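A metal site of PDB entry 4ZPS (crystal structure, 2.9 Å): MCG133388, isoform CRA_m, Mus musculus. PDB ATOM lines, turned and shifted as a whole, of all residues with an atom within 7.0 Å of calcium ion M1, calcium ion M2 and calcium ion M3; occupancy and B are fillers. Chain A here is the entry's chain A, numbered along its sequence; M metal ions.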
ATOM      1  N   ASN A 114     -37.333 -14.838 -26.583  1.00  0.00           N
ATOM      2  CA  ASN A 114     -36.288 -15.469 -25.789  1.00  0.00           C
ATOM      3  C   ASN A 114     -35.256 -16.148 -26.675  1.00  0.00           C
ATOM      4  O   ASN A 114     -35.569 -16.596 -27.770  1.00  0.00           O
ATOM      5  CB  ASN A 114     -36.909 -16.479 -24.814  1.00  0.00           C
ATOM      6  CG  ASN A 114     -35.944 -16.925 -23.733  1.00  0.00           C
ATOM      7  OD1 ASN A 114     -34.761 -17.144 -23.979  1.00  0.00           O
ATOM      8  ND2 ASN A 114     -36.451 -17.048 -22.513  1.00  0.00           N
ATOM      9  N   GLU A 115     -34.012 -16.220 -26.190  1.00  0.00           N
ATOM     10  CA  GLU A 115     -32.931 -16.863 -26.924  1.00  0.00           C
ATOM     11  C   GLU A 115     -33.210 -18.329 -27.209  1.00  0.00           C
ATOM     12  O   GLU A 115     -32.779 -18.860 -28.234  1.00  0.00           O
ATOM     13  CB  GLU A 115     -31.617 -16.766 -26.143  1.00  0.00           C
ATOM     14  CG  GLU A 115     -31.027 -15.389 -26.001  1.00  0.00           C
ATOM     15  CD  GLU A 115     -29.764 -15.423 -25.192  1.00  0.00           C
ATOM     16  OE1 GLU A 115     -29.694 -16.217 -24.233  1.00  0.00           O
ATOM     17  OE2 GLU A 115     -28.825 -14.660 -25.514  1.00  0.00           O
ATOM     18  N   LEU A 171     -31.364 -16.502 -31.893  1.00  0.00           N
ATOM     19  CA  LEU A 171     -30.914 -15.230 -31.327  1.00  0.00           C
ATOM     20  C   LEU A 171     -29.937 -15.471 -30.165  1.00  0.00           C
ATOM     21  O   LEU A 171     -29.799 -16.597 -29.681  1.00  0.00           O
ATOM     22  CB  LEU A 171     -32.107 -14.395 -30.850  1.00  0.00           C
ATOM     23  CG  LEU A 171     -33.057 -13.911 -31.954  1.00  0.00           C
ATOM     24  CD1 LEU A 171     -34.303 -13.274 -31.355  1.00  0.00           C
ATOM     25  CD2 LEU A 171     -32.358 -12.928 -32.871  1.00  0.00           C
ATOM     26  N   ASP A 172     -29.269 -14.401 -29.740  1.00  0.00           N
ATOM     27  CA  ASP A 172     -28.308 -14.476 -28.645  1.00  0.00           C
ATOM     28  C   ASP A 172     -28.055 -13.085 -28.072  1.00  0.00           C
ATOM     29  O   ASP A 172     -27.304 -12.298 -28.649  1.00  0.00           O
ATOM     30  CB  ASP A 172     -27.001 -15.112 -29.113  1.00  0.00           C
ATOM     31  CG  ASP A 172     -25.981 -15.252 -27.992  1.00  0.00           C
ATOM     32  OD1 ASP A 172     -26.390 -15.348 -26.816  1.00  0.00           O
ATOM     33  OD2 ASP A 172     -24.769 -15.273 -28.300  1.00  0.00           O
ATOM     34  N   ARG A 173     -28.674 -12.773 -26.929  1.00  0.00           N
ATOM     35  CA  ARG A 173     -28.537 -11.447 -26.332  1.00  0.00           C
ATOM     36  C   ARG A 173     -27.159 -11.247 -25.707  1.00  0.00           C
ATOM     37  O   ARG A 173     -26.771 -10.134 -25.367  1.00  0.00           O
ATOM     38  CB  ARG A 173     -29.630 -11.190 -25.292  1.00  0.00           C
ATOM     39  CG  ARG A 173     -29.498 -12.008 -24.026  1.00  0.00           C
ATOM     40  CD  ARG A 173     -29.995 -11.239 -22.808  1.00  0.00           C
ATOM     41  NE  ARG A 173     -29.124 -10.108 -22.493  1.00  0.00           N
ATOM     42  CZ  ARG A 173     -28.007 -10.203 -21.778  1.00  0.00           C
ATOM     43  NH1 ARG A 173     -27.620 -11.378 -21.312  1.00  0.00           N
ATOM     44  NH2 ARG A 173     -27.278  -9.123 -21.543  1.00  0.00           N
ATOM     45  N   GLU A 174     -26.425 -12.341 -25.540  1.00  0.00           N
ATOM     46  CA  GLU A 174     -25.048 -12.250 -25.062  1.00  0.00           C
ATOM     47  C   GLU A 174     -24.173 -11.612 -26.135  1.00  0.00           C
ATOM     48  O   GLU A 174     -23.083 -11.110 -25.848  1.00  0.00           O
ATOM     49  CB  GLU A 174     -24.504 -13.630 -24.669  1.00  0.00           C
ATOM     50  CG  GLU A 174     -24.889 -14.063 -23.261  1.00  0.00           C
ATOM     51  CD  GLU A 174     -26.355 -14.440 -23.124  1.00  0.00           C
ATOM     52  OE1 GLU A 174     -27.116 -13.671 -22.510  1.00  0.00           O
ATOM     53  OE2 GLU A 174     -26.739 -15.519 -23.628  1.00  0.00           O
ATOM     54  N   GLU A 175     -24.668 -11.622 -27.366  1.00  0.00           N
ATOM     55  CA  GLU A 175     -24.006 -10.946 -28.480  1.00  0.00           C
ATOM     56  C   GLU A 175     -24.740  -9.664 -28.864  1.00  0.00           C
ATOM     57  O   GLU A 175     -24.129  -8.600 -28.988  1.00  0.00           O
ATOM     58  CB  GLU A 175     -23.905 -11.878 -29.699  1.00  0.00           C
ATOM     59  CG  GLU A 175     -22.786 -12.892 -29.613  1.00  0.00           C
ATOM     60  CD  GLU A 175     -21.407 -12.258 -29.776  1.00  0.00           C
ATOM     61  OE1 GLU A 175     -21.337 -11.099 -30.228  1.00  0.00           O
ATOM     62  OE2 GLU A 175     -20.406 -12.927 -29.461  1.00  0.00           O
ATOM     63  N   LEU A 204     -35.067 -11.479 -24.914  1.00  0.00           N
ATOM     64  CA  LEU A 204     -35.088 -11.824 -23.501  1.00  0.00           C
ATOM     65  C   LEU A 204     -33.997 -12.843 -23.201  1.00  0.00           C
ATOM     66  O   LEU A 204     -33.505 -13.517 -24.100  1.00  0.00           O
ATOM     67  CB  LEU A 204     -36.454 -12.358 -23.086  1.00  0.00           C
ATOM     68  CG  LEU A 204     -37.635 -11.441 -23.399  1.00  0.00           C
ATOM     69  CD1 LEU A 204     -38.935 -11.996 -22.818  1.00  0.00           C
ATOM     70  CD2 LEU A 204     -37.383 -10.033 -22.897  1.00  0.00           C
ATOM     71  N   ASP A 205     -33.614 -12.949 -21.931  1.00  0.00           N
ATOM     72  CA  ASP A 205     -32.492 -13.799 -21.550  1.00  0.00           C
ATOM     73  C   ASP A 205     -32.912 -15.195 -21.123  1.00  0.00           C
ATOM     74  O   ASP A 205     -34.004 -15.389 -20.572  1.00  0.00           O
ATOM     75  CB  ASP A 205     -31.702 -13.142 -20.411  1.00  0.00           C
ATOM     76  CG  ASP A 205     -30.414 -13.889 -20.089  1.00  0.00           C
ATOM     77  OD1 ASP A 205     -29.381 -13.634 -20.743  1.00  0.00           O
ATOM     78  OD2 ASP A 205     -30.431 -14.736 -19.164  1.00  0.00           O
ATOM     79  N   THR A 206     -32.049 -16.161 -21.395  1.00  0.00           N
ATOM     80  CA  THR A 206     -32.160 -17.502 -20.816  1.00  0.00           C
ATOM     81  C   THR A 206     -30.803 -17.864 -20.221  1.00  0.00           C
ATOM     82  O   THR A 206     -29.770 -17.375 -20.667  1.00  0.00           O
ATOM     83  CB  THR A 206     -32.585 -18.550 -21.863  1.00  0.00           C
ATOM     84  OG1 THR A 206     -32.714 -19.833 -21.220  1.00  0.00           O
ATOM     85  CG2 THR A 206     -31.555 -18.650 -22.979  1.00  0.00           C
ATOM     86  N   ASN A 207     -30.816 -18.697 -19.191  1.00  0.00           N
ATOM     87  CA  ASN A 207     -29.581 -19.057 -18.488  1.00  0.00           C
ATOM     88  C   ASN A 207     -28.862 -20.220 -19.177  1.00  0.00           C
ATOM     89  O   ASN A 207     -28.976 -21.371 -18.750  1.00  0.00           O
ATOM     90  CB  ASN A 207     -29.884 -19.405 -17.032  1.00  0.00           C
ATOM     91  CG  ASN A 207     -28.637 -19.683 -16.232  1.00  0.00           C
ATOM     92  OD1 ASN A 207     -27.908 -18.772 -15.851  1.00  0.00           O
ATOM     93  ND2 ASN A 207     -28.383 -20.957 -15.960  1.00  0.00           N
ATOM     94  N   ASP A 208     -28.123 -19.910 -20.234  1.00  0.00           N
ATOM     95  CA  ASP A 208     -27.443 -20.933 -21.015  1.00  0.00           C
ATOM     96  C   ASP A 208     -25.926 -20.856 -20.866  1.00  0.00           C
ATOM     97  O   ASP A 208     -25.208 -21.781 -21.254  1.00  0.00           O
ATOM     98  CB  ASP A 208     -27.833 -20.822 -22.490  1.00  0.00           C
ATOM     99  CG  ASP A 208     -27.643 -19.428 -23.054  1.00  0.00           C
ATOM    100  OD1 ASP A 208     -27.765 -18.445 -22.289  1.00  0.00           O
ATOM    101  OD2 ASP A 208     -27.360 -19.303 -24.264  1.00  0.00           O
ATOM    102  N   ASN A 209     -25.438 -19.758 -20.307  1.00  0.00           N
ATOM    103  CA  ASN A 209     -24.008 -19.625 -20.033  1.00  0.00           C
ATOM    104  C   ASN A 209     -23.638 -20.073 -18.628  1.00  0.00           C
ATOM    105  O   ASN A 209     -24.025 -19.441 -17.644  1.00  0.00           O
ATOM    106  CB  ASN A 209     -23.553 -18.178 -20.258  1.00  0.00           C
ATOM    107  CG  ASN A 209     -23.446 -17.825 -21.720  1.00  0.00           C
ATOM    108  OD1 ASN A 209     -24.274 -17.072 -22.242  1.00  0.00           O
ATOM    109  ND2 ASN A 209     -22.434 -18.347 -22.393  1.00  0.00           N
ATOM    110  N   ALA A 210     -22.903 -21.170 -18.539  1.00  0.00           N
ATOM    111  CA  ALA A 210     -22.402 -21.664 -17.265  1.00  0.00           C
ATOM    112  C   ALA A 210     -21.152 -20.897 -16.866  1.00  0.00           C
ATOM    113  O   ALA A 210     -20.387 -20.452 -17.722  1.00  0.00           O
ATOM    114  CB  ALA A 210     -22.110 -23.156 -17.346  1.00  0.00           C
ATOM    115  N   PRO A 211     -20.937 -20.715 -15.553  1.00  0.00           N
ATOM    116  CA  PRO A 211     -19.740 -20.055 -15.028  1.00  0.00           C
ATOM    117  C   PRO A 211     -18.443 -20.699 -15.502  1.00  0.00           C
ATOM    118  O   PRO A 211     -18.310 -21.922 -15.449  1.00  0.00           O
ATOM    119  CB  PRO A 211     -19.895 -20.199 -13.509  1.00  0.00           C
ATOM    120  CG  PRO A 211     -21.367 -20.294 -13.299  1.00  0.00           C
ATOM    121  CD  PRO A 211     -21.894 -21.056 -14.485  1.00  0.00           C
ATOM    122  N   SER A 238     -16.389 -16.056 -15.527  1.00  0.00           N
ATOM    123  CA  SER A 238     -17.169 -15.299 -16.501  1.00  0.00           C
ATOM    124  C   SER A 238     -18.582 -15.875 -16.670  1.00  0.00           C
ATOM    125  O   SER A 238     -18.773 -17.086 -16.704  1.00  0.00           O
ATOM    126  CB  SER A 238     -16.464 -15.280 -17.848  1.00  0.00           C
ATOM    127  OG  SER A 238     -17.207 -14.552 -18.810  1.00  0.00           O
ATOM    128  N   ASP A 239     -19.556 -14.979 -16.779  1.00  0.00           N
ATOM    129  CA  ASP A 239     -20.947 -15.356 -17.002  1.00  0.00           C
ATOM    130  C   ASP A 239     -21.698 -14.193 -17.623  1.00  0.00           C
ATOM    131  O   ASP A 239     -22.158 -13.296 -16.908  1.00  0.00           O
ATOM    132  CB  ASP A 239     -21.601 -15.790 -15.687  1.00  0.00           C
ATOM    133  CG  ASP A 239     -22.807 -16.674 -15.902  1.00  0.00           C
ATOM    134  OD1 ASP A 239     -23.528 -16.478 -16.906  1.00  0.00           O
ATOM    135  OD2 ASP A 239     -23.041 -17.575 -15.066  1.00  0.00           O
ATOM    136  N   PRO A 240     -21.833 -14.189 -18.954  1.00  0.00           N
ATOM    137  CA  PRO A 240     -22.396 -13.075 -19.723  1.00  0.00           C
ATOM    138  C   PRO A 240     -23.909 -12.969 -19.620  1.00  0.00           C
ATOM    139  O   PRO A 240     -24.489 -12.029 -20.165  1.00  0.00           O
ATOM    140  CB  PRO A 240     -21.985 -13.401 -21.169  1.00  0.00           C
ATOM    141  CG  PRO A 240     -21.004 -14.535 -21.077  1.00  0.00           C
ATOM    142  CD  PRO A 240     -21.357 -15.270 -19.837  1.00  0.00           C
ATOM    143  N   ASP A 241     -24.546 -13.924 -18.935  1.00  0.00           N
ATOM    144  CA  ASP A 241     -25.998 -13.913 -18.785  1.00  0.00           C
ATOM    145  C   ASP A 241     -26.473 -12.663 -18.046  1.00  0.00           C
ATOM    146  O   ASP A 241     -25.693 -11.990 -17.382  1.00  0.00           O
ATOM    147  CB  ASP A 241     -26.465 -15.174 -18.059  1.00  0.00           C
ATOM    148  CG  ASP A 241     -26.245 -16.429 -18.877  1.00  0.00           C
ATOM    149  OD1 ASP A 241     -26.144 -16.323 -20.114  1.00  0.00           O
ATOM    150  OD2 ASP A 241     -26.178 -17.523 -18.274  1.00  0.00           O
ATOM    151  N   GLU A 242     -27.762 -12.371 -18.169  1.00  0.00           N
ATOM    152  CA  GLU A 242     -28.313 -11.121 -17.665  1.00  0.00           C
ATOM    153  C   GLU A 242     -28.677 -11.186 -16.181  1.00  0.00           C
ATOM    154  O   GLU A 242     -29.361 -12.108 -15.741  1.00  0.00           O
ATOM    155  CB  GLU A 242     -29.538 -10.716 -18.476  1.00  0.00           C
ATOM    156  CG  GLU A 242     -30.132  -9.368 -18.084  1.00  0.00           C
ATOM    157  CD  GLU A 242     -31.229  -8.926 -19.048  1.00  0.00           C
ATOM    158  OE1 GLU A 242     -31.596  -9.725 -19.934  1.00  0.00           O
ATOM    159  OE2 GLU A 242     -31.708  -7.779 -18.910  1.00  0.00           O
ATOM    160  N   VAL A 244     -29.481 -11.803 -12.673  1.00  0.00           N
ATOM    161  CA  VAL A 244     -29.473 -12.912 -11.731  1.00  0.00           C
ATOM    162  C   VAL A 244     -28.776 -14.138 -12.318  1.00  0.00           C
ATOM    163  O   VAL A 244     -28.076 -14.875 -11.615  1.00  0.00           O
ATOM    164  CB  VAL A 244     -30.909 -13.286 -11.306  1.00  0.00           C
ATOM    165  CG1 VAL A 244     -30.871 -14.250 -10.135  1.00  0.00           C
ATOM    166  CG2 VAL A 244     -31.690 -12.038 -10.940  1.00  0.00           C
ATOM    167  N   ASN A 245     -28.956 -14.359 -13.619  1.00  0.00           N
ATOM    168  CA  ASN A 245     -28.333 -15.468 -14.309  1.00  0.00           C
ATOM    169  C   ASN A 245     -26.824 -15.257 -14.503  1.00  0.00           C
ATOM    170  O   ASN A 245     -26.112 -16.172 -14.912  1.00  0.00           O
ATOM    171  CB  ASN A 245     -28.993 -15.700 -15.664  1.00  0.00           C
ATOM    172  CG  ASN A 245     -30.445 -16.102 -15.549  1.00  0.00           C
ATOM    173  OD1 ASN A 245     -30.827 -16.874 -14.668  1.00  0.00           O
ATOM    174  ND2 ASN A 245     -31.275 -15.577 -16.443  1.00  0.00           N
ATOM    175  N   GLY A 246     -26.366 -14.049 -14.206  1.00  0.00           N
ATOM    176  CA  GLY A 246     -24.957 -13.721 -14.366  1.00  0.00           C
ATOM    177  C   GLY A 246     -24.253 -13.572 -13.034  1.00  0.00           C
ATOM    178  O   GLY A 246     -23.033 -13.397 -12.984  1.00  0.00           O
ATOM    179  N   LYS A 247     -25.019 -13.639 -11.950  1.00  0.00           N
ATOM    180  CA  LYS A 247     -24.457 -13.569 -10.613  1.00  0.00           C
ATOM    181  C   LYS A 247     -23.673 -14.834 -10.297  1.00  0.00           C
ATOM    182  O   LYS A 247     -24.235 -15.921 -10.219  1.00  0.00           O
ATOM    183  CB  LYS A 247     -25.546 -13.355  -9.573  1.00  0.00           C
ATOM    184  CG  LYS A 247     -25.041 -13.247  -8.146  1.00  0.00           C
ATOM    185  CD  LYS A 247     -26.175 -13.024  -7.159  1.00  0.00           C
ATOM    186  CE  LYS A 247     -25.661 -13.032  -5.724  1.00  0.00           C
ATOM    187  NZ  LYS A 247     -26.750 -12.799  -4.741  1.00  0.00           N
ATOM    188  N   ASP A 294     -23.938 -20.320 -10.449  1.00  0.00           N
ATOM    189  CA  ASP A 294     -24.987 -19.329 -10.695  1.00  0.00           C
ATOM    190  C   ASP A 294     -26.329 -19.855 -10.182  1.00  0.00           C
ATOM    191  O   ASP A 294     -26.421 -20.989  -9.715  1.00  0.00           O
ATOM    192  CB  ASP A 294     -25.080 -18.981 -12.177  1.00  0.00           C
ATOM    193  CG  ASP A 294     -25.554 -20.143 -13.027  1.00  0.00           C
ATOM    194  OD1 ASP A 294     -25.456 -21.302 -12.567  1.00  0.00           O
ATOM    195  OD2 ASP A 294     -26.018 -19.900 -14.158  1.00  0.00           O
ATOM    196  N   VAL A 295     -27.373 -19.036 -10.292  1.00  0.00           N
ATOM    197  CA  VAL A 295     -28.674 -19.396  -9.757  1.00  0.00           C
ATOM    198  C   VAL A 295     -29.304 -20.579 -10.480  1.00  0.00           C
ATOM    199  O   VAL A 295     -30.227 -21.215  -9.963  1.00  0.00           O
ATOM    200  CB  VAL A 295     -29.645 -18.201  -9.815  1.00  0.00           C
ATOM    201  CG1 VAL A 295     -29.186 -17.103  -8.870  1.00  0.00           C
ATOM    202  CG2 VAL A 295     -29.765 -17.679 -11.240  1.00  0.00           C
ATOM    203  N   GLY A 296     -28.808 -20.874 -11.678  1.00  0.00           N
ATOM    204  CA  GLY A 296     -29.297 -22.009 -12.428  1.00  0.00           C
ATOM    205  C   GLY A 296     -28.580 -23.297 -12.057  1.00  0.00           C
ATOM    206  O   GLY A 296     -28.751 -24.320 -12.714  1.00  0.00           O
ATOM    207  N   LEU A 298     -25.511 -24.018 -12.387  1.00  0.00           N
ATOM    208  CA  LEU A 298     -24.494 -24.398 -13.354  1.00  0.00           C
ATOM    209  C   LEU A 298     -23.108 -24.191 -12.751  1.00  0.00           C
ATOM    210  O   LEU A 298     -22.829 -23.155 -12.153  1.00  0.00           O
ATOM    211  CB  LEU A 298     -24.632 -23.600 -14.649  1.00  0.00           C
ATOM    212  CG  LEU A 298     -25.962 -23.681 -15.393  1.00  0.00           C
ATOM    213  CD1 LEU A 298     -25.855 -22.943 -16.720  1.00  0.00           C
ATOM    214  CD2 LEU A 298     -26.397 -25.119 -15.617  1.00  0.00           C
HETATM  215 CA    CA M   1     -28.341 -15.636 -21.761  1.00  0.00          CA
HETATM  216 CA    CA M   2     -25.286 -18.218 -16.005  1.00  0.00          CA
HETATM  217 CA    CA M   3     -27.108 -17.175 -25.478  1.00  0.00          CA
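Calcium ion M3 is bound by the side-chain carboxylate (OD1) of Asp 172, the side-chain carboxylate (OD2) of Asp 208 and the side-chain carboxylate (OE2) of Glu 174.
Slightly farther from calcium ion M3 lies OE1 of Glu 115 (3.0 Å).
Slightly farther from calcium ion M3 lies OE2 of Glu 115 (3.0 Å).
The nearest printed residue that does not touch calcium ion M1 is Asn 209 (4.3 Å).
Calcium ion M1 is bound by the side-chain carboxylate (OE1) of Glu 174 (2.4 Å), the side-chain carboxylate (OE2) of Glu 174 (2.5 Å), the side-chain carboxylate (OD1) of Asp 205 (2.5 Å), the backbone carbonyl oxygen (O) of Thr 206 (2.5 Å), the side-chain carboxylate (OD1) of Asp 241 (2.8 Å) and the side-chain carboxylate (OE1) of Glu 115 (2.9 Å).
Calcium ion M1 has six donor atoms within binding distance.
Slightly farther from calcium ion M1 lies the side-chain carboxylate (OD1) of Asp 208 (2.9 Å).
Calcium ion M2 is bound by the backbone carbonyl oxygen (O) of Asn 209 (2.4 Å), the backbone carbonyl oxygen (O) of Asn 245 (2.5 Å), the side-chain carboxylate (OD2) of Asp 239 (2.5 Å), the side-chain carboxylate (OD2) of Asp 241 (2.5 Å), the side-chain carboxylate (OD2) of Asp 294 (2.6 Å), the side-chain carboxylate (OD1) of Asp 239 (2.6 Å) and the side-chain amide oxygen (OD1) of Asn 207 (2.7 Å).
Calcium ion M2 has seven donor atoms within binding distance.
Of the 28 residues printed, 6 come within 4 Å of calcium ion M2.
The side-chain amide oxygen (OD1) of Asn 209 lies close to the side-chain carboxylate (OE2) of Glu 174 (3.2 Å).
The guanidinium group (NH1) of Arg 173 sits close to the side-chain carboxylate (OE1) of Glu 174 (2.6 Å).
The side-chain carboxylate (OD2) of Asp 205 is in hydrogen-bond range of the side-chain amide nitrogen (ND2) of Asn 245.
NH1 of Arg 173 sits close to OD1 of Asp 205, at 2.9 Å.
The side-chain carboxylate (OD1) of Asp 205 sits close to the backbone NH (N) of Glu 242 (3.3 Å).
The backbone NH (N) of Leu 298 sits at hydrogen-bond distance from the side-chain carboxylate (OD1) of Asp 294 (2.7 Å).
The backbone NH of Gly 296 sits close to the side-chain carboxylate of Asp 294 (3.5 Å).
The backbone carbonyl oxygen (O) of Leu 204 sits at hydrogen-bond distance from the backbone NH (N) of Glu 115 (3.5 Å).
Within 4 Å of calcium ion M3: Glu 115, Asp 172, Glu 174 and Asp 208.
The nearest printed residue that does not touch calcium ion M3 is Asn 209 (4.3 Å).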
